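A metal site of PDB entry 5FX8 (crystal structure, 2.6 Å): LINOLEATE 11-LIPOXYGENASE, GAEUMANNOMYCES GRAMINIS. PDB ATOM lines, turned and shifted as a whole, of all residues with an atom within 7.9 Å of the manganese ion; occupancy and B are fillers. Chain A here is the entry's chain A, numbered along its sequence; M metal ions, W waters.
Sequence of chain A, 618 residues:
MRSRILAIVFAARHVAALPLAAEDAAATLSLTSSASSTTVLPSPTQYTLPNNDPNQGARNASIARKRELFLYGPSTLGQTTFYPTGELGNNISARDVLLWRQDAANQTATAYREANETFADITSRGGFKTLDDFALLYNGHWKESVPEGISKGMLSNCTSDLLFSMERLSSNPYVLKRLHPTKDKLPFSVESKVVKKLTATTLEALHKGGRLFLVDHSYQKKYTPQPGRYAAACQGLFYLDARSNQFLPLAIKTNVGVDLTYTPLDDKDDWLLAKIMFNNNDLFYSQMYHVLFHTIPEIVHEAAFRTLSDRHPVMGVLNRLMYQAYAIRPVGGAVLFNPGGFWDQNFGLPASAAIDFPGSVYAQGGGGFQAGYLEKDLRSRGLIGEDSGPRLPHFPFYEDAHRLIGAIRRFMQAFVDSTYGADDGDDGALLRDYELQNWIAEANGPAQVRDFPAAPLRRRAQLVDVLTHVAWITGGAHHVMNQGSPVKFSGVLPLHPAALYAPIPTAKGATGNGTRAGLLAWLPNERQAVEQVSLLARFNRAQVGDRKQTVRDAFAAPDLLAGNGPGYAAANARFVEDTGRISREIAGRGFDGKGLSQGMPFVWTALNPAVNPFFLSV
The manganese ion is bound by O of Val 618 (1.9 Å), NE2 of His 294 (2.1 Å), NE2 of His 478 (2.2 Å), OD1 of Asn 482 (2.4 Å), water W1 (2.4 Å) and NE2 of His 290 (2.4 Å).
A ring nitrogen (ND1) of His 478 lies within hydrogen-bond range of a ring nitrogen (ND1) of His 479 (3.0 Å). The side-chain amide nitrogen of Asn 482 sits at hydrogen-bond distance from the side-chain amide oxygen of Gln 287, at 2.9 Å. A ring nitrogen (ND1) of His 290 is in hydrogen-bond range of the backbone carbonyl oxygen (O) of Gln 287, at 2.7 Å.
Of the 16 residues printed, 5 come within 4 Å of the manganese ion.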
ATOM      1  N   GLN A 287     -22.203 -15.808 -33.734  1.00  0.00           N
ATOM      2  CA  GLN A 287     -23.297 -15.773 -32.786  1.00  0.00           C
ATOM      3  C   GLN A 287     -23.461 -17.111 -32.087  1.00  0.00           C
ATOM      4  O   GLN A 287     -23.855 -17.159 -30.928  1.00  0.00           O
ATOM      5  CB  GLN A 287     -24.590 -15.336 -33.478  1.00  0.00           C
ATOM      6  CG  GLN A 287     -24.551 -13.880 -33.905  1.00  0.00           C
ATOM      7  CD  GLN A 287     -23.744 -12.994 -32.938  1.00  0.00           C
ATOM      8  OE1 GLN A 287     -24.151 -12.763 -31.814  1.00  0.00           O
ATOM      9  NE2 GLN A 287     -22.577 -12.511 -33.393  1.00  0.00           N
ATOM     10  N   HIS A 290     -20.305 -18.192 -29.719  1.00  0.00           N
ATOM     11  CA  HIS A 290     -20.090 -17.471 -28.457  1.00  0.00           C
ATOM     12  C   HIS A 290     -20.964 -17.977 -27.314  1.00  0.00           C
ATOM     13  O   HIS A 290     -20.745 -17.578 -26.161  1.00  0.00           O
ATOM     14  CB  HIS A 290     -20.307 -15.956 -28.621  1.00  0.00           C
ATOM     15  CG  HIS A 290     -21.661 -15.472 -28.222  1.00  0.00           C
ATOM     16  ND1 HIS A 290     -22.763 -15.636 -29.030  1.00  0.00           N
ATOM     17  CD2 HIS A 290     -22.101 -14.799 -27.130  1.00  0.00           C
ATOM     18  CE1 HIS A 290     -23.818 -15.101 -28.450  1.00  0.00           C
ATOM     19  NE2 HIS A 290     -23.447 -14.589 -27.282  1.00  0.00           N
ATOM     20  N   VAL A 291     -21.950 -18.819 -27.607  1.00  0.00           N
ATOM     21  CA  VAL A 291     -22.647 -19.540 -26.552  1.00  0.00           C
ATOM     22  C   VAL A 291     -21.647 -20.158 -25.595  1.00  0.00           C
ATOM     23  O   VAL A 291     -21.830 -20.137 -24.368  1.00  0.00           O
ATOM     24  CB  VAL A 291     -23.589 -20.572 -27.171  1.00  0.00           C
ATOM     25  CG1 VAL A 291     -24.285 -21.399 -26.128  1.00  0.00           C
ATOM     26  CG2 VAL A 291     -24.577 -19.871 -27.988  1.00  0.00           C
ATOM     27  N   PHE A 293     -18.624 -18.950 -24.982  1.00  0.00           N
ATOM     28  CA  PHE A 293     -18.148 -17.866 -24.125  1.00  0.00           C
ATOM     29  C   PHE A 293     -19.118 -17.630 -22.975  1.00  0.00           C
ATOM     30  O   PHE A 293     -18.731 -17.059 -21.968  1.00  0.00           O
ATOM     31  CB  PHE A 293     -17.983 -16.539 -24.873  1.00  0.00           C
ATOM     32  CG  PHE A 293     -16.938 -16.536 -25.956  1.00  0.00           C
ATOM     33  CD1 PHE A 293     -16.263 -17.684 -26.322  1.00  0.00           C
ATOM     34  CD2 PHE A 293     -16.644 -15.377 -26.643  1.00  0.00           C
ATOM     35  CE1 PHE A 293     -15.325 -17.656 -27.326  1.00  0.00           C
ATOM     36  CE2 PHE A 293     -15.684 -15.358 -27.654  1.00  0.00           C
ATOM     37  CZ  PHE A 293     -15.048 -16.503 -27.988  1.00  0.00           C
ATOM     38  N   HIS A 294     -20.377 -18.037 -23.118  1.00  0.00           N
ATOM     39  CA  HIS A 294     -21.254 -17.951 -21.951  1.00  0.00           C
ATOM     40  C   HIS A 294     -21.119 -19.179 -21.041  1.00  0.00           C
ATOM     41  O   HIS A 294     -20.993 -19.024 -19.828  1.00  0.00           O
ATOM     42  CB  HIS A 294     -22.715 -17.777 -22.395  1.00  0.00           C
ATOM     43  CG  HIS A 294     -23.080 -16.377 -22.779  1.00  0.00           C
ATOM     44  ND1 HIS A 294     -23.373 -15.405 -21.853  1.00  0.00           N
ATOM     45  CD2 HIS A 294     -23.202 -15.791 -23.995  1.00  0.00           C
ATOM     46  CE1 HIS A 294     -23.661 -14.285 -22.473  1.00  0.00           C
ATOM     47  NE2 HIS A 294     -23.566 -14.486 -23.773  1.00  0.00           N
ATOM     48  N   ILE A 328     -28.623 -15.652 -19.056  1.00  0.00           N
ATOM     49  CA  ILE A 328     -28.512 -15.691 -20.519  1.00  0.00           C
ATOM     50  C   ILE A 328     -29.125 -16.971 -21.075  1.00  0.00           C
ATOM     51  O   ILE A 328     -29.807 -16.931 -22.102  1.00  0.00           O
ATOM     52  CB  ILE A 328     -27.048 -15.504 -20.969  1.00  0.00           C
ATOM     53  CG1 ILE A 328     -26.472 -14.206 -20.406  1.00  0.00           C
ATOM     54  CG2 ILE A 328     -26.951 -15.453 -22.481  1.00  0.00           C
ATOM     55  CD1 ILE A 328     -27.235 -12.991 -20.775  1.00  0.00           C
ATOM     56  N   LEU A 336     -35.227 -16.027 -27.582  1.00  0.00           N
ATOM     57  CA  LEU A 336     -34.332 -15.939 -28.718  1.00  0.00           C
ATOM     58  C   LEU A 336     -34.375 -17.175 -29.596  1.00  0.00           C
ATOM     59  O   LEU A 336     -34.606 -17.081 -30.796  1.00  0.00           O
ATOM     60  CB  LEU A 336     -32.905 -15.682 -28.216  1.00  0.00           C
ATOM     61  CG  LEU A 336     -31.808 -15.456 -29.246  1.00  0.00           C
ATOM     62  CD1 LEU A 336     -32.287 -14.416 -30.228  1.00  0.00           C
ATOM     63  CD2 LEU A 336     -30.569 -15.010 -28.533  1.00  0.00           C
ATOM     64  N   HIS A 478     -16.214 -11.877 -25.017  1.00  0.00           N
ATOM     65  CA  HIS A 478     -17.642 -11.849 -25.300  1.00  0.00           C
ATOM     66  C   HIS A 478     -18.013 -10.685 -26.197  1.00  0.00           C
ATOM     67  O   HIS A 478     -18.810 -10.832 -27.125  1.00  0.00           O
ATOM     68  CB  HIS A 478     -18.446 -11.749 -24.012  1.00  0.00           C
ATOM     69  CG  HIS A 478     -19.923 -11.653 -24.240  1.00  0.00           C
ATOM     70  ND1 HIS A 478     -20.558 -10.455 -24.466  1.00  0.00           N
ATOM     71  CD2 HIS A 478     -20.874 -12.603 -24.337  1.00  0.00           C
ATOM     72  CE1 HIS A 478     -21.847 -10.670 -24.658  1.00  0.00           C
ATOM     73  NE2 HIS A 478     -22.061 -11.964 -24.583  1.00  0.00           N
ATOM     74  N   HIS A 479     -17.430  -9.527 -25.946  1.00  0.00           N
ATOM     75  CA  HIS A 479     -17.876  -8.324 -26.626  1.00  0.00           C
ATOM     76  C   HIS A 479     -17.266  -8.185 -27.997  1.00  0.00           C
ATOM     77  O   HIS A 479     -17.581  -7.245 -28.719  1.00  0.00           O
ATOM     78  CB  HIS A 479     -17.571  -7.119 -25.741  1.00  0.00           C
ATOM     79  CG  HIS A 479     -17.937  -7.318 -24.296  1.00  0.00           C
ATOM     80  ND1 HIS A 479     -19.107  -7.925 -23.892  1.00  0.00           N
ATOM     81  CD2 HIS A 479     -17.285  -6.979 -23.163  1.00  0.00           C
ATOM     82  CE1 HIS A 479     -19.161  -7.941 -22.568  1.00  0.00           C
ATOM     83  NE2 HIS A 479     -18.067  -7.372 -22.115  1.00  0.00           N
ATOM     84  N   MET A 481     -17.542 -10.928 -30.049  1.00  0.00           N
ATOM     85  CA  MET A 481     -18.443 -11.763 -30.828  1.00  0.00           C
ATOM     86  C   MET A 481     -19.886 -11.285 -30.783  1.00  0.00           C
ATOM     87  O   MET A 481     -20.591 -11.352 -31.775  1.00  0.00           O
ATOM     88  CB  MET A 481     -18.387 -13.212 -30.325  1.00  0.00           C
ATOM     89  CG  MET A 481     -17.048 -13.888 -30.467  1.00  0.00           C
ATOM     90  SD  MET A 481     -16.651 -14.238 -32.176  1.00  0.00           S
ATOM     91  CE  MET A 481     -16.679 -16.023 -32.134  1.00  0.00           C
ATOM     92  N   ASN A 482     -20.319 -10.784 -29.637  1.00  0.00           N
ATOM     93  CA  ASN A 482     -21.706 -10.479 -29.331  1.00  0.00           C
ATOM     94  C   ASN A 482     -21.727  -9.054 -28.826  1.00  0.00           C
ATOM     95  O   ASN A 482     -20.949  -8.240 -29.313  1.00  0.00           O
ATOM     96  CB  ASN A 482     -22.233 -11.440 -28.277  1.00  0.00           C
ATOM     97  CG  ASN A 482     -23.715 -11.424 -28.164  1.00  0.00           C
ATOM     98  OD1 ASN A 482     -24.269 -11.440 -27.061  1.00  0.00           O
ATOM     99  ND2 ASN A 482     -24.391 -11.377 -29.303  1.00  0.00           N
ATOM    100  N   GLN A 483     -22.585  -8.743 -27.866  1.00  0.00           N
ATOM    101  CA  GLN A 483     -22.703  -7.405 -27.285  1.00  0.00           C
ATOM    102  C   GLN A 483     -22.942  -6.414 -28.428  1.00  0.00           C
ATOM    103  O   GLN A 483     -23.846  -6.639 -29.237  1.00  0.00           O
ATOM    104  CB  GLN A 483     -21.490  -7.137 -26.389  1.00  0.00           C
ATOM    105  CG  GLN A 483     -21.684  -6.043 -25.334  1.00  0.00           C
ATOM    106  CD  GLN A 483     -22.758  -6.320 -24.265  1.00  0.00           C
ATOM    107  OE1 GLN A 483     -22.787  -7.365 -23.612  1.00  0.00           O
ATOM    108  NE2 GLN A 483     -23.610  -5.359 -24.055  1.00  0.00           N
ATOM    109  N   PHE A 539     -28.927  -6.211 -28.812  1.00  0.00           N
ATOM    110  CA  PHE A 539     -27.809  -6.863 -28.117  1.00  0.00           C
ATOM    111  C   PHE A 539     -26.845  -5.863 -27.464  1.00  0.00           C
ATOM    112  O   PHE A 539     -26.018  -6.262 -26.648  1.00  0.00           O
ATOM    113  CB  PHE A 539     -27.026  -7.747 -29.075  1.00  0.00           C
ATOM    114  CG  PHE A 539     -27.779  -8.923 -29.602  1.00  0.00           C
ATOM    115  CD1 PHE A 539     -28.957  -9.339 -29.023  1.00  0.00           C
ATOM    116  CD2 PHE A 539     -27.298  -9.641 -30.681  1.00  0.00           C
ATOM    117  CE1 PHE A 539     -29.620 -10.425 -29.515  1.00  0.00           C
ATOM    118  CE2 PHE A 539     -27.967 -10.726 -31.165  1.00  0.00           C
ATOM    119  CZ  PHE A 539     -29.124 -11.116 -30.572  1.00  0.00           C
ATOM    120  N   LEU A 616     -21.108 -10.579 -18.622  1.00  0.00           N
ATOM    121  CA  LEU A 616     -21.772 -11.164 -19.785  1.00  0.00           C
ATOM    122  C   LEU A 616     -23.225 -10.681 -19.812  1.00  0.00           C
ATOM    123  O   LEU A 616     -24.128 -11.329 -19.305  1.00  0.00           O
ATOM    124  CB  LEU A 616     -21.686 -12.690 -19.749  1.00  0.00           C
ATOM    125  CG  LEU A 616     -20.313 -13.394 -19.706  1.00  0.00           C
ATOM    126  CD1 LEU A 616     -20.437 -14.820 -19.195  1.00  0.00           C
ATOM    127  CD2 LEU A 616     -19.576 -13.414 -21.019  1.00  0.00           C
ATOM    128  N   SER A 617     -23.458  -9.525 -20.432  1.00  0.00           N
ATOM    129  CA  SER A 617     -24.725  -8.827 -20.275  1.00  0.00           C
ATOM    130  C   SER A 617     -25.811  -9.283 -21.251  1.00  0.00           C
ATOM    131  O   SER A 617     -27.000  -9.075 -20.968  1.00  0.00           O
ATOM    132  CB  SER A 617     -24.517  -7.321 -20.368  1.00  0.00           C
ATOM    133  OG  SER A 617     -24.361  -6.870 -21.679  1.00  0.00           O
ATOM    134  N   VAL A 618     -25.463  -9.921 -22.370  1.00  0.00           N
ATOM    135  CA  VAL A 618     -26.476 -10.458 -23.278  1.00  0.00           C
ATOM    136  C   VAL A 618     -26.092 -11.819 -23.861  1.00  0.00           C
ATOM    137  O   VAL A 618     -24.906 -12.091 -24.152  1.00  0.00           O
ATOM    138  CB  VAL A 618     -26.771  -9.459 -24.402  1.00  0.00           C
ATOM    139  CG1 VAL A 618     -27.528  -8.264 -23.876  1.00  0.00           C
ATOM    140  CG2 VAL A 618     -25.486  -8.999 -25.069  1.00  0.00           C
HETATM  141 MN    MN M   1     -23.811 -13.101 -25.372  1.00  0.00          MN
HETATM  142  O   HOH W   1     -25.943 -13.931 -26.209  1.00  0.00           O
